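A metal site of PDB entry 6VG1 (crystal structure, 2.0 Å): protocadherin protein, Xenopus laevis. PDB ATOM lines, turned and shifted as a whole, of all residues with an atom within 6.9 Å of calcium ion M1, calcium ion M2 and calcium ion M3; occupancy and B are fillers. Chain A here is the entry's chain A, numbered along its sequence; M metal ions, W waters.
The backbone NH (N) of Arg 172 sits close to the side-chain carboxylate (OE1) of Glu 114 (3.0 Å). N of Glu 114 sits at hydrogen-bond distance from O of Leu 203, at 3.0 Å. The guanidinium group (NH2) of Arg 172 sits close to the side-chain carboxylate (OE2) of Glu 173 (3.5 Å). The side-chain carboxylate (OD2) of Asp 204 sits at hydrogen-bond distance from the side-chain amide nitrogen (ND2) of Asn 244 (3.1 Å). OD1 of Asp 204 lies close to NE of Arg 172. The side-chain carboxylate (OD2) of Asp 204 sits at hydrogen-bond distance from the backbone NH (N) of Glu 241. The side-chain carboxylate of Asp 294 is in hydrogen-bond range of the backbone NH of Leu 300 (2.7 Å). The side-chain hydroxyl (OG) of Ser 174 sits at hydrogen-bond distance from the side-chain carboxylate (OD2) of Asp 171, at 3.1 Å.
Within 4 Å of calcium ion M2: Asn 206, Asn 208, Asp 238, Asp 240, Asn 244 and Asp 294.
Of the 26 residues printed, 5 come within 4 Å of calcium ion M3.
The side-chain carboxylate (OE2) of Glu 173 binds calcium ion M1 (2.3 Å). The side-chain carboxylate (OE2) of Glu 114 binds calcium ion M1, 2.4 Å away. The side-chain carboxylate (OD1) of Asp 204 is bound to calcium ion M1, 2.4 Å away. Calcium ion M1 is bound by the side-chain carboxylate (OD1) of Asp 207 (2.4 Å). The side-chain carboxylate (OD2) of Asp 240 is bound to calcium ion M1 (2.4 Å). O of Phe 205 is bound to calcium ion M1, 2.4 Å away. Slightly farther from calcium ion M1 lies the side-chain carboxylate (OE1) of Glu 173 (3.0 Å).
Calcium ion M2 is bound by O of Asn 208 (2.3 Å), OD2 of Asp 294 (2.4 Å), OD1 of Asp 240 (2.4 Å), OD1 of Asp 238 (2.4 Å), O of Asn 244 (2.4 Å), OD1 of Asn 206 (2.4 Å) and OD2 of Asp 238 (2.4 Å). Calcium ion M2 has seven donor atoms within binding distance.
Calcium ion M3 is bound by OD2 of Asp 207 (2.2 Å), water W1 (2.3 Å), OE1 of Glu 114 (2.3 Å), OE1 of Glu 173 (2.3 Å), OD1 of Asp 171 (2.5 Å) and water W2 (2.6 Å). Slightly farther from calcium ion M3 lies OD1 of Asp 207 (3.1 Å).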
ATOM      1  N   GLU A 114      12.416   1.569   6.050  1.00  0.00           N
ATOM      2  CA  GLU A 114      12.251   0.466   6.996  1.00  0.00           C
ATOM      3  C   GLU A 114      13.547   0.176   7.742  1.00  0.00           C
ATOM      4  O   GLU A 114      13.517  -0.504   8.777  1.00  0.00           O
ATOM      5  CB  GLU A 114      11.765  -0.790   6.279  1.00  0.00           C
ATOM      6  CG  GLU A 114      12.833  -1.587   5.570  1.00  0.00           C
ATOM      7  CD  GLU A 114      12.237  -2.810   4.885  1.00  0.00           C
ATOM      8  OE1 GLU A 114      11.635  -3.657   5.585  1.00  0.00           O
ATOM      9  OE2 GLU A 114      12.360  -2.912   3.638  1.00  0.00           O
ATOM     10  N   LEU A 170      10.843  -0.991  11.862  1.00  0.00           N
ATOM     11  CA  LEU A 170       9.837  -1.165  10.825  1.00  0.00           C
ATOM     12  C   LEU A 170      10.168  -2.358   9.924  1.00  0.00           C
ATOM     13  O   LEU A 170      11.313  -2.797   9.840  1.00  0.00           O
ATOM     14  CB  LEU A 170       9.695   0.087   9.959  1.00  0.00           C
ATOM     15  CG  LEU A 170       9.140   1.333  10.631  1.00  0.00           C
ATOM     16  CD1 LEU A 170       9.137   2.466   9.620  1.00  0.00           C
ATOM     17  CD2 LEU A 170       7.766   1.123  11.211  1.00  0.00           C
ATOM     18  N   ASP A 171       9.136  -2.863   9.235  1.00  0.00           N
ATOM     19  CA  ASP A 171       9.285  -3.923   8.235  1.00  0.00           C
ATOM     20  C   ASP A 171       8.259  -3.635   7.150  1.00  0.00           C
ATOM     21  O   ASP A 171       7.069  -3.910   7.326  1.00  0.00           O
ATOM     22  CB  ASP A 171       9.084  -5.305   8.856  1.00  0.00           C
ATOM     23  CG  ASP A 171       9.288  -6.424   7.841  1.00  0.00           C
ATOM     24  OD1 ASP A 171       9.742  -6.141   6.708  1.00  0.00           O
ATOM     25  OD2 ASP A 171       9.009  -7.597   8.199  1.00  0.00           O
ATOM     26  N   ARG A 172       8.735  -3.130   6.003  1.00  0.00           N
ATOM     27  CA  ARG A 172       7.801  -2.766   4.933  1.00  0.00           C
ATOM     28  C   ARG A 172       7.045  -3.969   4.397  1.00  0.00           C
ATOM     29  O   ARG A 172       5.940  -3.814   3.866  1.00  0.00           O
ATOM     30  CB  ARG A 172       8.553  -2.063   3.795  1.00  0.00           C
ATOM     31  CG  ARG A 172       7.632  -1.344   2.819  1.00  0.00           C
ATOM     32  CD  ARG A 172       8.251  -1.200   1.435  1.00  0.00           C
ATOM     33  NE  ARG A 172       8.472  -2.507   0.803  1.00  0.00           N
ATOM     34  CZ  ARG A 172       7.581  -3.115   0.024  1.00  0.00           C
ATOM     35  NH1 ARG A 172       6.414  -2.553  -0.238  1.00  0.00           N
ATOM     36  NH2 ARG A 172       7.876  -4.292  -0.503  1.00  0.00           N
ATOM     37  N   GLU A 173       7.613  -5.169   4.502  1.00  0.00           N
ATOM     38  CA  GLU A 173       6.933  -6.356   4.004  1.00  0.00           C
ATOM     39  C   GLU A 173       5.753  -6.739   4.895  1.00  0.00           C
ATOM     40  O   GLU A 173       4.781  -7.318   4.416  1.00  0.00           O
ATOM     41  CB  GLU A 173       7.925  -7.508   3.882  1.00  0.00           C
ATOM     42  CG  GLU A 173       8.916  -7.364   2.712  1.00  0.00           C
ATOM     43  CD  GLU A 173       9.824  -6.148   2.829  1.00  0.00           C
ATOM     44  OE1 GLU A 173      10.140  -5.744   3.961  1.00  0.00           O
ATOM     45  OE2 GLU A 173      10.215  -5.597   1.772  1.00  0.00           O
ATOM     46  N   SER A 174       5.829  -6.431   6.203  1.00  0.00           N
ATOM     47  CA  SER A 174       4.698  -6.623   7.095  1.00  0.00           C
ATOM     48  C   SER A 174       3.690  -5.488   6.966  1.00  0.00           C
ATOM     49  O   SER A 174       2.484  -5.722   6.850  1.00  0.00           O
ATOM     50  CB  SER A 174       5.176  -6.733   8.550  1.00  0.00           C
ATOM     51  OG  SER A 174       5.949  -7.898   8.773  1.00  0.00           O
ATOM     52  N   LEU A 203       9.535   3.328   3.185  1.00  0.00           N
ATOM     53  CA  LEU A 203      10.352   3.141   2.005  1.00  0.00           C
ATOM     54  C   LEU A 203      11.152   1.853   2.107  1.00  0.00           C
ATOM     55  O   LEU A 203      11.637   1.496   3.184  1.00  0.00           O
ATOM     56  CB  LEU A 203      11.312   4.322   1.822  1.00  0.00           C
ATOM     57  CG  LEU A 203      10.644   5.693   1.703  1.00  0.00           C
ATOM     58  CD1 LEU A 203      11.714   6.766   1.556  1.00  0.00           C
ATOM     59  CD2 LEU A 203       9.678   5.743   0.544  1.00  0.00           C
ATOM     60  N   ASP A 204      11.287   1.150   0.977  1.00  0.00           N
ATOM     61  CA  ASP A 204      11.815  -0.205   1.020  1.00  0.00           C
ATOM     62  C   ASP A 204      13.336  -0.216   1.104  1.00  0.00           C
ATOM     63  O   ASP A 204      14.018   0.615   0.487  1.00  0.00           O
ATOM     64  CB  ASP A 204      11.375  -1.018  -0.192  1.00  0.00           C
ATOM     65  CG  ASP A 204      11.818  -2.479  -0.108  1.00  0.00           C
ATOM     66  OD1 ASP A 204      11.284  -3.211   0.745  1.00  0.00           O
ATOM     67  OD2 ASP A 204      12.687  -2.889  -0.914  1.00  0.00           O
ATOM     68  N   PHE A 205      13.856  -1.152   1.881  1.00  0.00           N
ATOM     69  CA  PHE A 205      15.259  -1.531   1.906  1.00  0.00           C
ATOM     70  C   PHE A 205      15.356  -2.951   1.369  1.00  0.00           C
ATOM     71  O   PHE A 205      14.395  -3.726   1.460  1.00  0.00           O
ATOM     72  CB  PHE A 205      15.808  -1.432   3.332  1.00  0.00           C
ATOM     73  CG  PHE A 205      17.280  -1.705   3.437  1.00  0.00           C
ATOM     74  CD1 PHE A 205      18.208  -0.905   2.780  1.00  0.00           C
ATOM     75  CD2 PHE A 205      17.741  -2.742   4.219  1.00  0.00           C
ATOM     76  CE1 PHE A 205      19.559  -1.157   2.886  1.00  0.00           C
ATOM     77  CE2 PHE A 205      19.089  -2.999   4.333  1.00  0.00           C
ATOM     78  CZ  PHE A 205      19.998  -2.206   3.667  1.00  0.00           C
ATOM     79  N   ASN A 206      16.501  -3.287   0.776  1.00  0.00           N
ATOM     80  CA  ASN A 206      16.705  -4.623   0.206  1.00  0.00           C
ATOM     81  C   ASN A 206      17.254  -5.548   1.292  1.00  0.00           C
ATOM     82  O   ASN A 206      18.426  -5.906   1.311  1.00  0.00           O
ATOM     83  CB  ASN A 206      17.633  -4.564  -0.998  1.00  0.00           C
ATOM     84  CG  ASN A 206      17.740  -5.901  -1.709  1.00  0.00           C
ATOM     85  OD1 ASN A 206      16.739  -6.579  -1.948  1.00  0.00           O
ATOM     86  ND2 ASN A 206      18.963  -6.292  -2.034  1.00  0.00           N
ATOM     87  N   ASP A 207      16.360  -5.911   2.213  1.00  0.00           N
ATOM     88  CA  ASP A 207      16.700  -6.771   3.330  1.00  0.00           C
ATOM     89  C   ASP A 207      16.167  -8.181   3.165  1.00  0.00           C
ATOM     90  O   ASP A 207      16.174  -8.957   4.131  1.00  0.00           O
ATOM     91  CB  ASP A 207      16.165  -6.163   4.627  1.00  0.00           C
ATOM     92  CG  ASP A 207      14.698  -5.779   4.519  1.00  0.00           C
ATOM     93  OD1 ASP A 207      14.185  -5.646   3.384  1.00  0.00           O
ATOM     94  OD2 ASP A 207      14.063  -5.585   5.592  1.00  0.00           O
ATOM     95  N   ASN A 208      15.736  -8.549   1.962  1.00  0.00           N
ATOM     96  CA  ASN A 208      15.284  -9.902   1.686  1.00  0.00           C
ATOM     97  C   ASN A 208      15.966 -10.413   0.441  1.00  0.00           C
ATOM     98  O   ASN A 208      15.755  -9.893  -0.656  1.00  0.00           O
ATOM     99  CB  ASN A 208      13.760  -9.942   1.532  1.00  0.00           C
ATOM    100  CG  ASN A 208      13.050  -9.859   2.851  1.00  0.00           C
ATOM    101  OD1 ASN A 208      12.401  -8.866   3.161  1.00  0.00           O
ATOM    102  ND2 ASN A 208      13.180 -10.913   3.648  1.00  0.00           N
ATOM    103  N   SER A 209      16.759 -11.473   0.593  1.00  0.00           N
ATOM    104  CA  SER A 209      17.332 -12.147  -0.543  1.00  0.00           C
ATOM    105  C   SER A 209      16.251 -12.981  -1.219  1.00  0.00           C
ATOM    106  O   SER A 209      15.276 -13.379  -0.576  1.00  0.00           O
ATOM    107  CB  SER A 209      18.463 -13.055  -0.090  1.00  0.00           C
ATOM    108  OG  SER A 209      18.070 -13.725   1.103  1.00  0.00           O
ATOM    109  N   PRO A 210      16.390 -13.246  -2.516  1.00  0.00           N
ATOM    110  CA  PRO A 210      15.415 -14.123  -3.184  1.00  0.00           C
ATOM    111  C   PRO A 210      15.455 -15.527  -2.589  1.00  0.00           C
ATOM    112  O   PRO A 210      16.385 -15.896  -1.865  1.00  0.00           O
ATOM    113  CB  PRO A 210      15.860 -14.131  -4.653  1.00  0.00           C
ATOM    114  CG  PRO A 210      17.237 -13.540  -4.663  1.00  0.00           C
ATOM    115  CD  PRO A 210      17.373 -12.671  -3.449  1.00  0.00           C
ATOM    116  N   ASP A 238      10.908 -12.803  -4.473  1.00  0.00           N
ATOM    117  CA  ASP A 238      11.569 -11.815  -3.620  1.00  0.00           C
ATOM    118  C   ASP A 238      10.489 -10.881  -3.077  1.00  0.00           C
ATOM    119  O   ASP A 238       9.773 -10.255  -3.872  1.00  0.00           O
ATOM    120  CB  ASP A 238      12.614 -11.011  -4.392  1.00  0.00           C
ATOM    121  CG  ASP A 238      13.599 -10.284  -3.473  1.00  0.00           C
ATOM    122  OD1 ASP A 238      14.781 -10.683  -3.426  1.00  0.00           O
ATOM    123  OD2 ASP A 238      13.186  -9.303  -2.820  1.00  0.00           O
ATOM    124  N   PRO A 239      10.329 -10.767  -1.766  1.00  0.00           N
ATOM    125  CA  PRO A 239       9.232  -9.925  -1.238  1.00  0.00           C
ATOM    126  C   PRO A 239       9.483  -8.432  -1.383  1.00  0.00           C
ATOM    127  O   PRO A 239       8.523  -7.664  -1.298  1.00  0.00           O
ATOM    128  CB  PRO A 239       9.145 -10.347   0.235  1.00  0.00           C
ATOM    129  CG  PRO A 239      10.544 -10.781   0.576  1.00  0.00           C
ATOM    130  CD  PRO A 239      11.091 -11.426  -0.679  1.00  0.00           C
ATOM    131  N   ASP A 240      10.732  -8.017  -1.602  1.00  0.00           N
ATOM    132  CA  ASP A 240      11.064  -6.592  -1.655  1.00  0.00           C
ATOM    133  C   ASP A 240      10.335  -5.931  -2.823  1.00  0.00           C
ATOM    134  O   ASP A 240       9.709  -6.576  -3.652  1.00  0.00           O
ATOM    135  CB  ASP A 240      12.578  -6.401  -1.795  1.00  0.00           C
ATOM    136  CG  ASP A 240      13.376  -6.851  -0.553  1.00  0.00           C
ATOM    137  OD1 ASP A 240      14.355  -7.618  -0.724  1.00  0.00           O
ATOM    138  OD2 ASP A 240      13.034  -6.441   0.588  1.00  0.00           O
ATOM    139  N   GLU A 241      10.463  -4.602  -2.885  1.00  0.00           N
ATOM    140  CA  GLU A 241       9.685  -3.773  -3.805  1.00  0.00           C
ATOM    141  C   GLU A 241      10.502  -3.436  -5.043  1.00  0.00           C
ATOM    142  O   GLU A 241      11.722  -3.296  -4.991  1.00  0.00           O
ATOM    143  CB  GLU A 241       9.228  -2.476  -3.127  1.00  0.00           C
ATOM    144  CG  GLU A 241       8.430  -1.556  -4.032  1.00  0.00           C
ATOM    145  CD  GLU A 241       8.074  -0.238  -3.351  1.00  0.00           C
ATOM    146  OE1 GLU A 241       8.218  -0.140  -2.103  1.00  0.00           O
ATOM    147  OE2 GLU A 241       7.655   0.711  -4.049  1.00  0.00           O
ATOM    148  N   ALA A 243      12.754  -2.879  -8.014  1.00  0.00           N
ATOM    149  CA  ALA A 243      13.983  -3.526  -8.471  1.00  0.00           C
ATOM    150  C   ALA A 243      14.540  -4.472  -7.405  1.00  0.00           C
ATOM    151  O   ALA A 243      15.101  -5.518  -7.729  1.00  0.00           O
ATOM    152  CB  ALA A 243      15.027  -2.469  -8.838  1.00  0.00           C
ATOM    153  N   ASN A 244      14.405  -4.111  -6.129  1.00  0.00           N
ATOM    154  CA  ASN A 244      14.922  -4.974  -5.079  1.00  0.00           C
ATOM    155  C   ASN A 244      14.268  -6.349  -5.055  1.00  0.00           C
ATOM    156  O   ASN A 244      14.773  -7.258  -4.406  1.00  0.00           O
ATOM    157  CB  ASN A 244      14.739  -4.329  -3.704  1.00  0.00           C
ATOM    158  CG  ASN A 244      15.575  -3.079  -3.556  1.00  0.00           C
ATOM    159  OD1 ASN A 244      16.496  -2.846  -4.337  1.00  0.00           O
ATOM    160  ND2 ASN A 244      15.271  -2.272  -2.558  1.00  0.00           N
ATOM    161  N   GLY A 245      13.152  -6.519  -5.766  1.00  0.00           N
ATOM    162  CA  GLY A 245      12.446  -7.773  -5.778  1.00  0.00           C
ATOM    163  C   GLY A 245      12.385  -8.398  -7.164  1.00  0.00           C
ATOM    164  O   GLY A 245      11.695  -9.402  -7.372  1.00  0.00           O
ATOM    165  N   GLU A 246      13.088  -7.782  -8.117  1.00  0.00           N
ATOM    166  CA  GLU A 246      13.115  -8.249  -9.495  1.00  0.00           C
ATOM    167  C   GLU A 246      14.309  -9.181  -9.664  1.00  0.00           C
ATOM    168  O   GLU A 246      15.446  -8.783  -9.374  1.00  0.00           O
ATOM    169  CB  GLU A 246      13.194  -7.057 -10.456  1.00  0.00           C
ATOM    170  CG  GLU A 246      12.801  -7.366 -11.894  1.00  0.00           C
ATOM    171  CD  GLU A 246      12.639  -6.110 -12.742  1.00  0.00           C
ATOM    172  OE1 GLU A 246      12.781  -4.993 -12.194  1.00  0.00           O
ATOM    173  OE2 GLU A 246      12.360  -6.246 -13.953  1.00  0.00           O
ATOM    174  N   ASP A 294      18.615 -10.533  -7.054  1.00  0.00           N
ATOM    175  CA  ASP A 294      17.757  -9.370  -7.244  1.00  0.00           C
ATOM    176  C   ASP A 294      18.574  -8.214  -7.818  1.00  0.00           C
ATOM    177  O   ASP A 294      19.791  -8.143  -7.640  1.00  0.00           O
ATOM    178  CB  ASP A 294      17.073  -8.937  -5.944  1.00  0.00           C
ATOM    179  CG  ASP A 294      18.048  -8.589  -4.833  1.00  0.00           C
ATOM    180  OD1 ASP A 294      19.257  -8.451  -5.104  1.00  0.00           O
ATOM    181  OD2 ASP A 294      17.587  -8.469  -3.680  1.00  0.00           O
ATOM    182  N   MET A 295      17.886  -7.300  -8.502  1.00  0.00           N
ATOM    183  CA  MET A 295      18.547  -6.167  -9.142  1.00  0.00           C
ATOM    184  C   MET A 295      18.459  -4.962  -8.215  1.00  0.00           C
ATOM    185  O   MET A 295      17.645  -4.051  -8.376  1.00  0.00           O
ATOM    186  CB  MET A 295      17.920  -5.895 -10.503  1.00  0.00           C
ATOM    187  CG  MET A 295      18.230  -6.969 -11.512  1.00  0.00           C
ATOM    188  SD  MET A 295      17.529  -6.622 -13.131  1.00  0.00           S
ATOM    189  CE  MET A 295      15.785  -6.900 -12.774  1.00  0.00           C
ATOM    190  N   ALA A 296      19.327  -4.980  -7.204  1.00  0.00           N
ATOM    191  CA  ALA A 296      19.389  -3.916  -6.213  1.00  0.00           C
ATOM    192  C   ALA A 296      20.818  -3.401  -6.108  1.00  0.00           C
ATOM    193  O   ALA A 296      21.771  -3.998  -6.627  1.00  0.00           O
ATOM    194  CB  ALA A 296      18.900  -4.394  -4.840  1.00  0.00           C
ATOM    195  N   LEU A 300      21.293  -9.365  -3.590  1.00  0.00           N
ATOM    196  CA  LEU A 300      21.162 -10.564  -2.772  1.00  0.00           C
ATOM    197  C   LEU A 300      20.924 -11.763  -3.681  1.00  0.00           C
ATOM    198  O   LEU A 300      20.343 -11.645  -4.761  1.00  0.00           O
ATOM    199  CB  LEU A 300      20.020 -10.401  -1.782  1.00  0.00           C
ATOM    200  CG  LEU A 300      20.211  -9.203  -0.840  1.00  0.00           C
ATOM    201  CD1 LEU A 300      19.011  -8.900   0.008  1.00  0.00           C
ATOM    202  CD2 LEU A 300      21.461  -9.481   0.024  1.00  0.00           C
HETATM  203 CA    CA M   1      12.332  -4.765   2.178  1.00  0.00          CA
HETATM  204 CA    CA M   2      15.508  -8.583  -2.561  1.00  0.00          CA
HETATM  205 CA    CA M   3      11.875  -5.907   5.500  1.00  0.00          CA
HETATM  206  O   HOH W   1      12.055  -5.683   7.741  1.00  0.00           O
HETATM  207  O   HOH W   2      11.699  -8.464   5.933  1.00  0.00           O
